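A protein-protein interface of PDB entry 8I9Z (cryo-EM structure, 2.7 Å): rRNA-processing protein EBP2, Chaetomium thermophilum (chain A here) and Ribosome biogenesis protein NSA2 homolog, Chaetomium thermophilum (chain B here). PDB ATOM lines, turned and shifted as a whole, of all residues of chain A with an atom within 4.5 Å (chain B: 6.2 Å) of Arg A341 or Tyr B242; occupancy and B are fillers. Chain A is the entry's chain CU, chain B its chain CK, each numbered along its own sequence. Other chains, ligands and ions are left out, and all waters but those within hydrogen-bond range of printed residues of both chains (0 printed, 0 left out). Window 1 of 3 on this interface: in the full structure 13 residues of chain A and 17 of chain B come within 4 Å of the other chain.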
ATOM      1  N   LEU A 337     -30.826 -23.093  19.078  1.00  0.00           N
ATOM      2  CA  LEU A 337     -30.258 -24.110  18.201  1.00  0.00           C
ATOM      3  C   LEU A 337     -31.043 -25.410  18.285  1.00  0.00           C
ATOM      4  O   LEU A 337     -31.244 -26.086  17.271  1.00  0.00           O
ATOM      5  CB  LEU A 337     -28.796 -24.356  18.561  1.00  0.00           C
ATOM      6  CG  LEU A 337     -28.017 -25.255  17.607  1.00  0.00           C
ATOM      7  CD1 LEU A 337     -28.198 -24.812  16.165  1.00  0.00           C
ATOM      8  CD2 LEU A 337     -26.552 -25.297  17.983  1.00  0.00           C
ATOM      9  N   LYS A 338     -31.481 -25.781  19.489  1.00  0.00           N
ATOM     10  CA  LYS A 338     -32.171 -27.052  19.682  1.00  0.00           C
ATOM     11  C   LYS A 338     -33.519 -27.065  18.975  1.00  0.00           C
ATOM     12  O   LYS A 338     -33.908 -28.072  18.373  1.00  0.00           O
ATOM     13  CB  LYS A 338     -32.339 -27.324  21.176  1.00  0.00           C
ATOM     14  CG  LYS A 338     -32.630 -28.768  21.524  1.00  0.00           C
ATOM     15  CD  LYS A 338     -32.568 -28.992  23.025  1.00  0.00           C
ATOM     16  CE  LYS A 338     -33.852 -29.611  23.542  1.00  0.00           C
ATOM     17  NZ  LYS A 338     -33.675 -31.048  23.879  1.00  0.00           N
ATOM     18  N   ARG A 339     -34.247 -25.949  19.034  1.00  0.00           N
ATOM     19  CA  ARG A 339     -35.537 -25.869  18.356  1.00  0.00           C
ATOM     20  C   ARG A 339     -35.362 -25.784  16.847  1.00  0.00           C
ATOM     21  O   ARG A 339     -36.219 -26.248  16.088  1.00  0.00           O
ATOM     22  CB  ARG A 339     -36.325 -24.667  18.869  1.00  0.00           C
ATOM     23  CG  ARG A 339     -37.356 -25.000  19.928  1.00  0.00           C
ATOM     24  CD  ARG A 339     -37.856 -23.740  20.618  1.00  0.00           C
ATOM     25  NE  ARG A 339     -38.316 -23.992  21.980  1.00  0.00           N
ATOM     26  CZ  ARG A 339     -37.521 -24.192  23.023  1.00  0.00           C
ATOM     27  NH1 ARG A 339     -36.204 -24.157  22.909  1.00  0.00           N
ATOM     28  NH2 ARG A 339     -38.064 -24.426  24.215  1.00  0.00           N
ATOM     29  N   LYS A 340     -34.261 -25.181  16.397  1.00  0.00           N
ATOM     30  CA  LYS A 340     -34.036 -25.002  14.967  1.00  0.00           C
ATOM     31  C   LYS A 340     -33.758 -26.325  14.270  1.00  0.00           C
ATOM     32  O   LYS A 340     -34.263 -26.573  13.170  1.00  0.00           O
ATOM     33  CB  LYS A 340     -32.877 -24.038  14.747  1.00  0.00           C
ATOM     34  CG  LYS A 340     -32.833 -23.446  13.370  1.00  0.00           C
ATOM     35  CD  LYS A 340     -31.637 -22.546  13.225  1.00  0.00           C
ATOM     36  CE  LYS A 340     -32.061 -21.196  12.706  1.00  0.00           C
ATOM     37  NZ  LYS A 340     -33.319 -21.262  11.910  1.00  0.00           N
ATOM     38  N   ARG A 341     -32.945 -27.181  14.888  1.00  0.00           N
ATOM     39  CA  ARG A 341     -32.634 -28.473  14.290  1.00  0.00           C
ATOM     40  C   ARG A 341     -33.843 -29.398  14.322  1.00  0.00           C
ATOM     41  O   ARG A 341     -34.025 -30.226  13.422  1.00  0.00           O
ATOM     42  CB  ARG A 341     -31.455 -29.109  15.021  1.00  0.00           C
ATOM     43  CG  ARG A 341     -30.213 -28.249  15.059  1.00  0.00           C
ATOM     44  CD  ARG A 341     -29.099 -28.839  14.239  1.00  0.00           C
ATOM     45  NE  ARG A 341     -27.828 -28.183  14.516  1.00  0.00           N
ATOM     46  CZ  ARG A 341     -26.711 -28.820  14.832  1.00  0.00           C
ATOM     47  NH1 ARG A 341     -26.672 -30.138  14.924  1.00  0.00           N
ATOM     48  NH2 ARG A 341     -25.605 -28.119  15.052  1.00  0.00           N
ATOM     49  N   ALA A 342     -34.672 -29.282  15.361  1.00  0.00           N
ATOM     50  CA  ALA A 342     -35.889 -30.081  15.438  1.00  0.00           C
ATOM     51  C   ALA A 342     -36.899 -29.653  14.383  1.00  0.00           C
ATOM     52  O   ALA A 342     -37.600 -30.494  13.808  1.00  0.00           O
ATOM     53  CB  ALA A 342     -36.497 -29.977  16.835  1.00  0.00           C
ATOM     54  N   GLU A 343     -37.000 -28.348  14.126  1.00  0.00           N
ATOM     55  CA  GLU A 343     -37.914 -27.866  13.098  1.00  0.00           C
ATOM     56  C   GLU A 343     -37.434 -28.255  11.706  1.00  0.00           C
ATOM     57  O   GLU A 343     -38.246 -28.571  10.828  1.00  0.00           O
ATOM     58  CB  GLU A 343     -38.080 -26.353  13.214  1.00  0.00           C
ATOM     59  CG  GLU A 343     -39.166 -25.932  14.194  1.00  0.00           C
ATOM     60  CD  GLU A 343     -38.775 -24.725  15.023  1.00  0.00           C
ATOM     61  OE1 GLU A 343     -37.824 -24.016  14.632  1.00  0.00           O
ATOM     62  OE2 GLU A 343     -39.418 -24.486  16.067  1.00  0.00           O
ATOM     63  N   GLY A 344     -36.125 -28.234  11.480  1.00  0.00           N
ATOM     64  CA  GLY A 344     -35.571 -28.660  10.212  1.00  0.00           C
ATOM     65  C   GLY A 344     -34.058 -28.700  10.218  1.00  0.00           C
ATOM     66  O   GLY A 344     -33.409 -27.740  10.640  1.00  0.00           O
ATOM     67  N   GLY A 345     -33.482 -29.802   9.752  1.00  0.00           N
ATOM     68  CA  GLY A 345     -32.039 -29.933   9.690  1.00  0.00           C
ATOM     69  C   GLY A 345     -31.423 -30.482  10.961  1.00  0.00           C
ATOM     70  O   GLY A 345     -30.628 -31.419  10.920  1.00  0.00           O
ATOM     71  N   LEU A 349     -26.775 -30.414   7.256  1.00  0.00           N
ATOM     72  CA  LEU A 349     -25.450 -30.303   7.846  1.00  0.00           C
ATOM     73  C   LEU A 349     -24.483 -31.219   7.103  1.00  0.00           C
ATOM     74  O   LEU A 349     -24.864 -31.962   6.197  1.00  0.00           O
ATOM     75  CB  LEU A 349     -25.484 -30.653   9.336  1.00  0.00           C
ATOM     76  CG  LEU A 349     -25.851 -29.558  10.334  1.00  0.00           C
ATOM     77  CD1 LEU A 349     -27.358 -29.408  10.447  1.00  0.00           C
ATOM     78  CD2 LEU A 349     -25.243 -29.868  11.689  1.00  0.00           C
ATOM     79  N   GLU A 353     -19.237 -31.818  12.535  1.00  0.00           N
ATOM     80  CA  GLU A 353     -19.561 -30.468  12.968  1.00  0.00           C
ATOM     81  C   GLU A 353     -18.512 -29.483  12.467  1.00  0.00           C
ATOM     82  O   GLU A 353     -17.393 -29.859  12.111  1.00  0.00           O
ATOM     83  CB  GLU A 353     -19.653 -30.412  14.493  1.00  0.00           C
ATOM     84  CG  GLU A 353     -21.042 -30.672  15.094  1.00  0.00           C
ATOM     85  CD  GLU A 353     -22.172 -29.801  14.546  1.00  0.00           C
ATOM     86  OE1 GLU A 353     -23.340 -30.213  14.705  1.00  0.00           O
ATOM     87  OE2 GLU A 353     -21.925 -28.687  14.035  1.00  0.00           O
ATOM     88  N   PHE A 358     -17.911 -22.383  19.362  1.00  0.00           N
ATOM     89  CA  PHE A 358     -19.238 -21.923  19.731  1.00  0.00           C
ATOM     90  C   PHE A 358     -19.291 -20.401  19.776  1.00  0.00           C
ATOM     91  O   PHE A 358     -18.265 -19.719  19.863  1.00  0.00           O
ATOM     92  CB  PHE A 358     -19.651 -22.516  21.077  1.00  0.00           C
ATOM     93  CG  PHE A 358     -20.490 -23.745  20.951  1.00  0.00           C
ATOM     94  CD1 PHE A 358     -21.850 -23.691  21.192  1.00  0.00           C
ATOM     95  CD2 PHE A 358     -19.932 -24.939  20.547  1.00  0.00           C
ATOM     96  CE1 PHE A 358     -22.631 -24.810  21.059  1.00  0.00           C
ATOM     97  CE2 PHE A 358     -20.710 -26.063  20.411  1.00  0.00           C
ATOM     98  CZ  PHE A 358     -22.062 -25.997  20.666  1.00  0.00           C
ATOM     99  N   ALA A 361     -20.129 -20.684  15.310  1.00  0.00           N
ATOM    100  CA  ALA A 361     -20.899 -21.646  14.530  1.00  0.00           C
ATOM    101  C   ALA A 361     -22.389 -21.524  14.822  1.00  0.00           C
ATOM    102  O   ALA A 361     -23.220 -21.720  13.929  1.00  0.00           O
ATOM    103  CB  ALA A 361     -20.406 -23.063  14.811  1.00  0.00           C
ATOM    104  N   GLU A 365     -25.275 -20.289  12.206  1.00  0.00           N
ATOM    105  CA  GLU A 365     -26.511 -21.027  11.969  1.00  0.00           C
ATOM    106  C   GLU A 365     -27.735 -20.149  12.181  1.00  0.00           C
ATOM    107  O   GLU A 365     -28.762 -20.336  11.521  1.00  0.00           O
ATOM    108  CB  GLU A 365     -26.578 -22.254  12.871  1.00  0.00           C
ATOM    109  CG  GLU A 365     -25.673 -23.388  12.444  1.00  0.00           C
ATOM    110  CD  GLU A 365     -26.377 -24.728  12.485  1.00  0.00           C
ATOM    111  OE1 GLU A 365     -27.619 -24.752  12.354  1.00  0.00           O
ATOM    112  OE2 GLU A 365     -25.690 -25.758  12.650  1.00  0.00           O
ATOM    113  N   LYS B 201     -17.248 -29.136  24.000  1.00  0.00           N
ATOM    114  CA  LYS B 201     -17.298 -27.941  23.169  1.00  0.00           C
ATOM    115  C   LYS B 201     -17.661 -26.684  23.947  1.00  0.00           C
ATOM    116  O   LYS B 201     -17.060 -25.629  23.731  1.00  0.00           O
ATOM    117  CB  LYS B 201     -18.288 -28.144  22.022  1.00  0.00           C
ATOM    118  CG  LYS B 201     -17.799 -29.107  20.960  1.00  0.00           C
ATOM    119  CD  LYS B 201     -17.020 -28.377  19.884  1.00  0.00           C
ATOM    120  CE  LYS B 201     -16.926 -29.199  18.618  1.00  0.00           C
ATOM    121  NZ  LYS B 201     -16.301 -30.522  18.880  1.00  0.00           N
ATOM    122  N   ILE B 220     -22.425 -28.885  26.061  1.00  0.00           N
ATOM    123  CA  ILE B 220     -22.430 -29.480  24.732  1.00  0.00           C
ATOM    124  C   ILE B 220     -21.157 -30.290  24.540  1.00  0.00           C
ATOM    125  O   ILE B 220     -20.051 -29.809  24.808  1.00  0.00           O
ATOM    126  CB  ILE B 220     -22.567 -28.406  23.646  1.00  0.00           C
ATOM    127  CG1 ILE B 220     -23.726 -27.462  23.957  1.00  0.00           C
ATOM    128  CG2 ILE B 220     -22.785 -29.064  22.298  1.00  0.00           C
ATOM    129  CD1 ILE B 220     -25.059 -28.150  24.093  1.00  0.00           C
ATOM    130  N   ILE B 221     -21.316 -31.527  24.083  1.00  0.00           N
ATOM    131  CA  ILE B 221     -20.209 -32.400  23.731  1.00  0.00           C
ATOM    132  C   ILE B 221     -20.449 -32.902  22.317  1.00  0.00           C
ATOM    133  O   ILE B 221     -21.570 -32.878  21.806  1.00  0.00           O
ATOM    134  CB  ILE B 221     -20.062 -33.581  24.710  1.00  0.00           C
ATOM    135  CG1 ILE B 221     -21.380 -34.343  24.815  1.00  0.00           C
ATOM    136  CG2 ILE B 221     -19.619 -33.093  26.072  1.00  0.00           C
ATOM    137  CD1 ILE B 221     -21.288 -35.606  25.611  1.00  0.00           C
ATOM    138  N   GLU B 222     -19.376 -33.348  21.678  1.00  0.00           N
ATOM    139  CA  GLU B 222     -19.437 -33.884  20.326  1.00  0.00           C
ATOM    140  C   GLU B 222     -19.257 -35.393  20.397  1.00  0.00           C
ATOM    141  O   GLU B 222     -18.267 -35.877  20.954  1.00  0.00           O
ATOM    142  CB  GLU B 222     -18.373 -33.239  19.442  1.00  0.00           C
ATOM    143  CG  GLU B 222     -18.645 -33.340  17.956  1.00  0.00           C
ATOM    144  CD  GLU B 222     -17.381 -33.228  17.126  1.00  0.00           C
ATOM    145  OE1 GLU B 222     -16.413 -33.962  17.404  1.00  0.00           O
ATOM    146  OE2 GLU B 222     -17.354 -32.397  16.193  1.00  0.00           O
ATOM    147  N   VAL B 223     -20.212 -36.131  19.841  1.00  0.00           N
ATOM    148  CA  VAL B 223     -20.232 -37.581  19.958  1.00  0.00           C
ATOM    149  C   VAL B 223     -20.111 -38.190  18.573  1.00  0.00           C
ATOM    150  O   VAL B 223     -20.460 -37.572  17.563  1.00  0.00           O
ATOM    151  CB  VAL B 223     -21.506 -38.093  20.665  1.00  0.00           C
ATOM    152  CG1 VAL B 223     -21.553 -37.588  22.089  1.00  0.00           C
ATOM    153  CG2 VAL B 223     -22.743 -37.665  19.908  1.00  0.00           C
ATOM    154  N   GLY B 240     -20.061 -36.792  13.447  1.00  0.00           N
ATOM    155  CA  GLY B 240     -19.928 -36.037  14.672  1.00  0.00           C
ATOM    156  C   GLY B 240     -21.089 -35.093  14.870  1.00  0.00           C
ATOM    157  O   GLY B 240     -21.373 -34.270  13.997  1.00  0.00           O
ATOM    158  N   ARG B 241     -21.759 -35.184  16.015  1.00  0.00           N
ATOM    159  CA  ARG B 241     -22.951 -34.392  16.267  1.00  0.00           C
ATOM    160  C   ARG B 241     -22.892 -33.780  17.658  1.00  0.00           C
ATOM    161  O   ARG B 241     -22.226 -34.290  18.560  1.00  0.00           O
ATOM    162  CB  ARG B 241     -24.223 -35.230  16.125  1.00  0.00           C
ATOM    163  CG  ARG B 241     -25.176 -34.734  15.064  1.00  0.00           C
ATOM    164  CD  ARG B 241     -24.531 -34.803  13.713  1.00  0.00           C
ATOM    165  NE  ARG B 241     -25.420 -34.363  12.649  1.00  0.00           N
ATOM    166  CZ  ARG B 241     -25.039 -34.179  11.394  1.00  0.00           C
ATOM    167  NH1 ARG B 241     -23.785 -34.365  11.020  1.00  0.00           N
ATOM    168  NH2 ARG B 241     -25.939 -33.802  10.493  1.00  0.00           N
ATOM    169  N   TYR B 242     -23.603 -32.669  17.815  1.00  0.00           N
ATOM    170  CA  TYR B 242     -23.725 -32.013  19.109  1.00  0.00           C
ATOM    171  C   TYR B 242     -24.699 -32.765  20.005  1.00  0.00           C
ATOM    172  O   TYR B 242     -25.743 -33.240  19.553  1.00  0.00           O
ATOM    173  CB  TYR B 242     -24.214 -30.577  18.929  1.00  0.00           C
ATOM    174  CG  TYR B 242     -23.179 -29.603  18.431  1.00  0.00           C
ATOM    175  CD1 TYR B 242     -21.828 -29.832  18.623  1.00  0.00           C
ATOM    176  CD2 TYR B 242     -23.559 -28.448  17.766  1.00  0.00           C
ATOM    177  CE1 TYR B 242     -20.885 -28.935  18.170  1.00  0.00           C
ATOM    178  CE2 TYR B 242     -22.627 -27.550  17.310  1.00  0.00           C
ATOM    179  CZ  TYR B 242     -21.292 -27.798  17.514  1.00  0.00           C
ATOM    180  OH  TYR B 242     -20.359 -26.901  17.056  1.00  0.00           O
ATOM    181  N   ALA B 243     -24.362 -32.857  21.287  1.00  0.00           N
ATOM    182  CA  ALA B 243     -25.240 -33.447  22.287  1.00  0.00           C
ATOM    183  C   ALA B 243     -25.141 -32.633  23.566  1.00  0.00           C
ATOM    184  O   ALA B 243     -24.038 -32.273  23.989  1.00  0.00           O
ATOM    185  CB  ALA B 243     -24.876 -34.907  22.554  1.00  0.00           C
ATOM    186  N   GLN B 244     -26.283 -32.349  24.178  1.00  0.00           N
ATOM    187  CA  GLN B 244     -26.345 -31.588  25.418  1.00  0.00           C
ATOM    188  C   GLN B 244     -26.484 -32.548  26.591  1.00  0.00           C
ATOM    189  O   GLN B 244     -27.395 -33.380  26.606  1.00  0.00           O
ATOM    190  CB  GLN B 244     -27.515 -30.608  25.393  1.00  0.00           C
ATOM    191  CG  GLN B 244     -27.737 -29.881  26.698  1.00  0.00           C
ATOM    192  CD  GLN B 244     -28.258 -28.482  26.500  1.00  0.00           C
ATOM    193  OE1 GLN B 244     -27.633 -27.510  26.911  1.00  0.00           O
ATOM    194  NE2 GLN B 244     -29.417 -28.370  25.866  1.00  0.00           N
ATOM    195  N   VAL B 258     -28.646 -35.770  25.078  1.00  0.00           N
ATOM    196  CA  VAL B 258     -29.647 -35.785  24.018  1.00  0.00           C
ATOM    197  C   VAL B 258     -29.043 -35.105  22.800  1.00  0.00           C
ATOM    198  O   VAL B 258     -28.473 -34.014  22.916  1.00  0.00           O
ATOM    199  CB  VAL B 258     -30.947 -35.084  24.453  1.00  0.00           C
ATOM    200  CG1 VAL B 258     -31.966 -35.110  23.338  1.00  0.00           C
ATOM    201  CG2 VAL B 258     -31.516 -35.734  25.699  1.00  0.00           C
ATOM    202  N   LEU B 259     -29.151 -35.754  21.642  1.00  0.00           N
ATOM    203  CA  LEU B 259     -28.575 -35.226  20.412  1.00  0.00           C
ATOM    204  C   LEU B 259     -29.301 -33.961  19.978  1.00  0.00           C
ATOM    205  O   LEU B 259     -30.529 -33.875  20.061  1.00  0.00           O
ATOM    206  CB  LEU B 259     -28.650 -36.270  19.298  1.00  0.00           C
ATOM    207  CG  LEU B 259     -27.468 -37.217  19.107  1.00  0.00           C
ATOM    208  CD1 LEU B 259     -27.665 -38.075  17.876  1.00  0.00           C
ATOM    209  CD2 LEU B 259     -26.176 -36.458  19.017  1.00  0.00           C
ATOM    210  N   LEU B 260     -28.538 -32.977  19.509  1.00  0.00           N
ATOM    211  CA  LEU B 260     -29.109 -31.739  18.997  1.00  0.00           C
ATOM    212  C   LEU B 260     -29.426 -31.870  17.513  1.00  0.00           C
ATOM    213  O   LEU B 260     -28.973 -31.056  16.704  1.00  0.00           O
ATOM    214  CB  LEU B 260     -28.154 -30.569  19.226  1.00  0.00           C
ATOM    215  CG  LEU B 260     -28.330 -29.759  20.507  1.00  0.00           C
ATOM    216  CD1 LEU B 260     -27.543 -30.386  21.639  1.00  0.00           C
ATOM    217  CD2 LEU B 260     -27.903 -28.322  20.292  1.00  0.00           C
ATOM    218  N   VAL B 261     -30.198 -32.887  17.147  1.00  0.00           N
ATOM    219  CA  VAL B 261     -30.551 -33.111  15.754  1.00  0.00           C
ATOM    220  C   VAL B 261     -31.978 -32.652  15.497  1.00  0.00           C
ATOM    221  O   VAL B 261     -32.759 -32.469  16.430  1.00  0.00           O
ATOM    222  CB  VAL B 261     -30.378 -34.585  15.367  1.00  0.00           C
ATOM    223  CG1 VAL B 261     -28.917 -34.894  15.107  1.00  0.00           C
ATOM    224  CG2 VAL B 261     -30.935 -35.486  16.452  1.00  0.00           C
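The backbone carbonyl oxygen (O) of Leu B260 is in hydrogen-bond range of the guanidinium group (NH1) of Arg A341, at 3.1 Å.
The backbone NH of Lys B201 lies within hydrogen-bond range of the backbone carbonyl oxygen of Ile B220. NZ of Lys B201 is in salt-bridge range of OE2 of Glu B222 (3.4 Å). N of Val B223 sits at hydrogen-bond distance from O of Arg B241. The backbone carbonyl oxygen (O) of Tyr B242 lies within hydrogen-bond range of the backbone NH (N) of Leu B260, at 2.8 Å. The guanidinium group of Arg A341 is in salt-bridge range of the side-chain carboxylate of Glu A353 (3.1 Å). OE2 of Glu A365 is in salt-bridge range of NH2 of Arg A341, at 3.4 Å.
Among the printed residues, pairs that only touch across the chains: Arg A341 with Tyr B242 (3.4 Å), Arg A341 with Val B261 (3.6 Å), Ala A342 with Val B261 (3.9 Å), Leu A349 with Arg B241 (3.4 Å), Glu A353 with Glu B222 (3.5 Å), Glu A353 with Gly B240 (3.6 Å), Glu A353 with Tyr B242 (3.5 Å), Phe A358 with Lys B201 (3.6 Å), Phe A358 with Ile B220 (3.5 Å) and Phe A358 with Tyr B242 (3.4 Å).
Of the printed residues of chain B, Arg A341 touches Tyr B242 (3.4 Å), Leu B260 (3.1 Å) and Val B261 (3.6 Å). Of the printed residues of chain A, Glu B222 touches Glu A353 (3.5 Å). Printed residues of chain A within 4 Å of Arg B241: Leu A349 (3.4 Å). Of chain A, only Arg A341 (3.4 Å), Glu A353 (3.5 Å) and Phe A358 (3.4 Å) come within 4 Å of Tyr B242. Of the printed residues of chain A, Val B261 touches Arg A341 and Ala A342.
Printed residues of chain A that touch a printed residue of chain B: Arg A341, Ala A342, Leu A349, Glu A353 and Phe A358. Hydrophobic or aromatic side chains of chain A that line the printed part of chain B: Leu A349 and Phe A358. Hydrophobic or aromatic side chains of chain B within 4 Å of the printed part of chain A: Ile B220 and Tyr B242. Among the printed residues, 11 pairs touch across the chains. Among the printed residues, no Asp or Glu carboxylate lies within 4 Å of a Lys or Arg side-chain nitrogen of the other chain.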
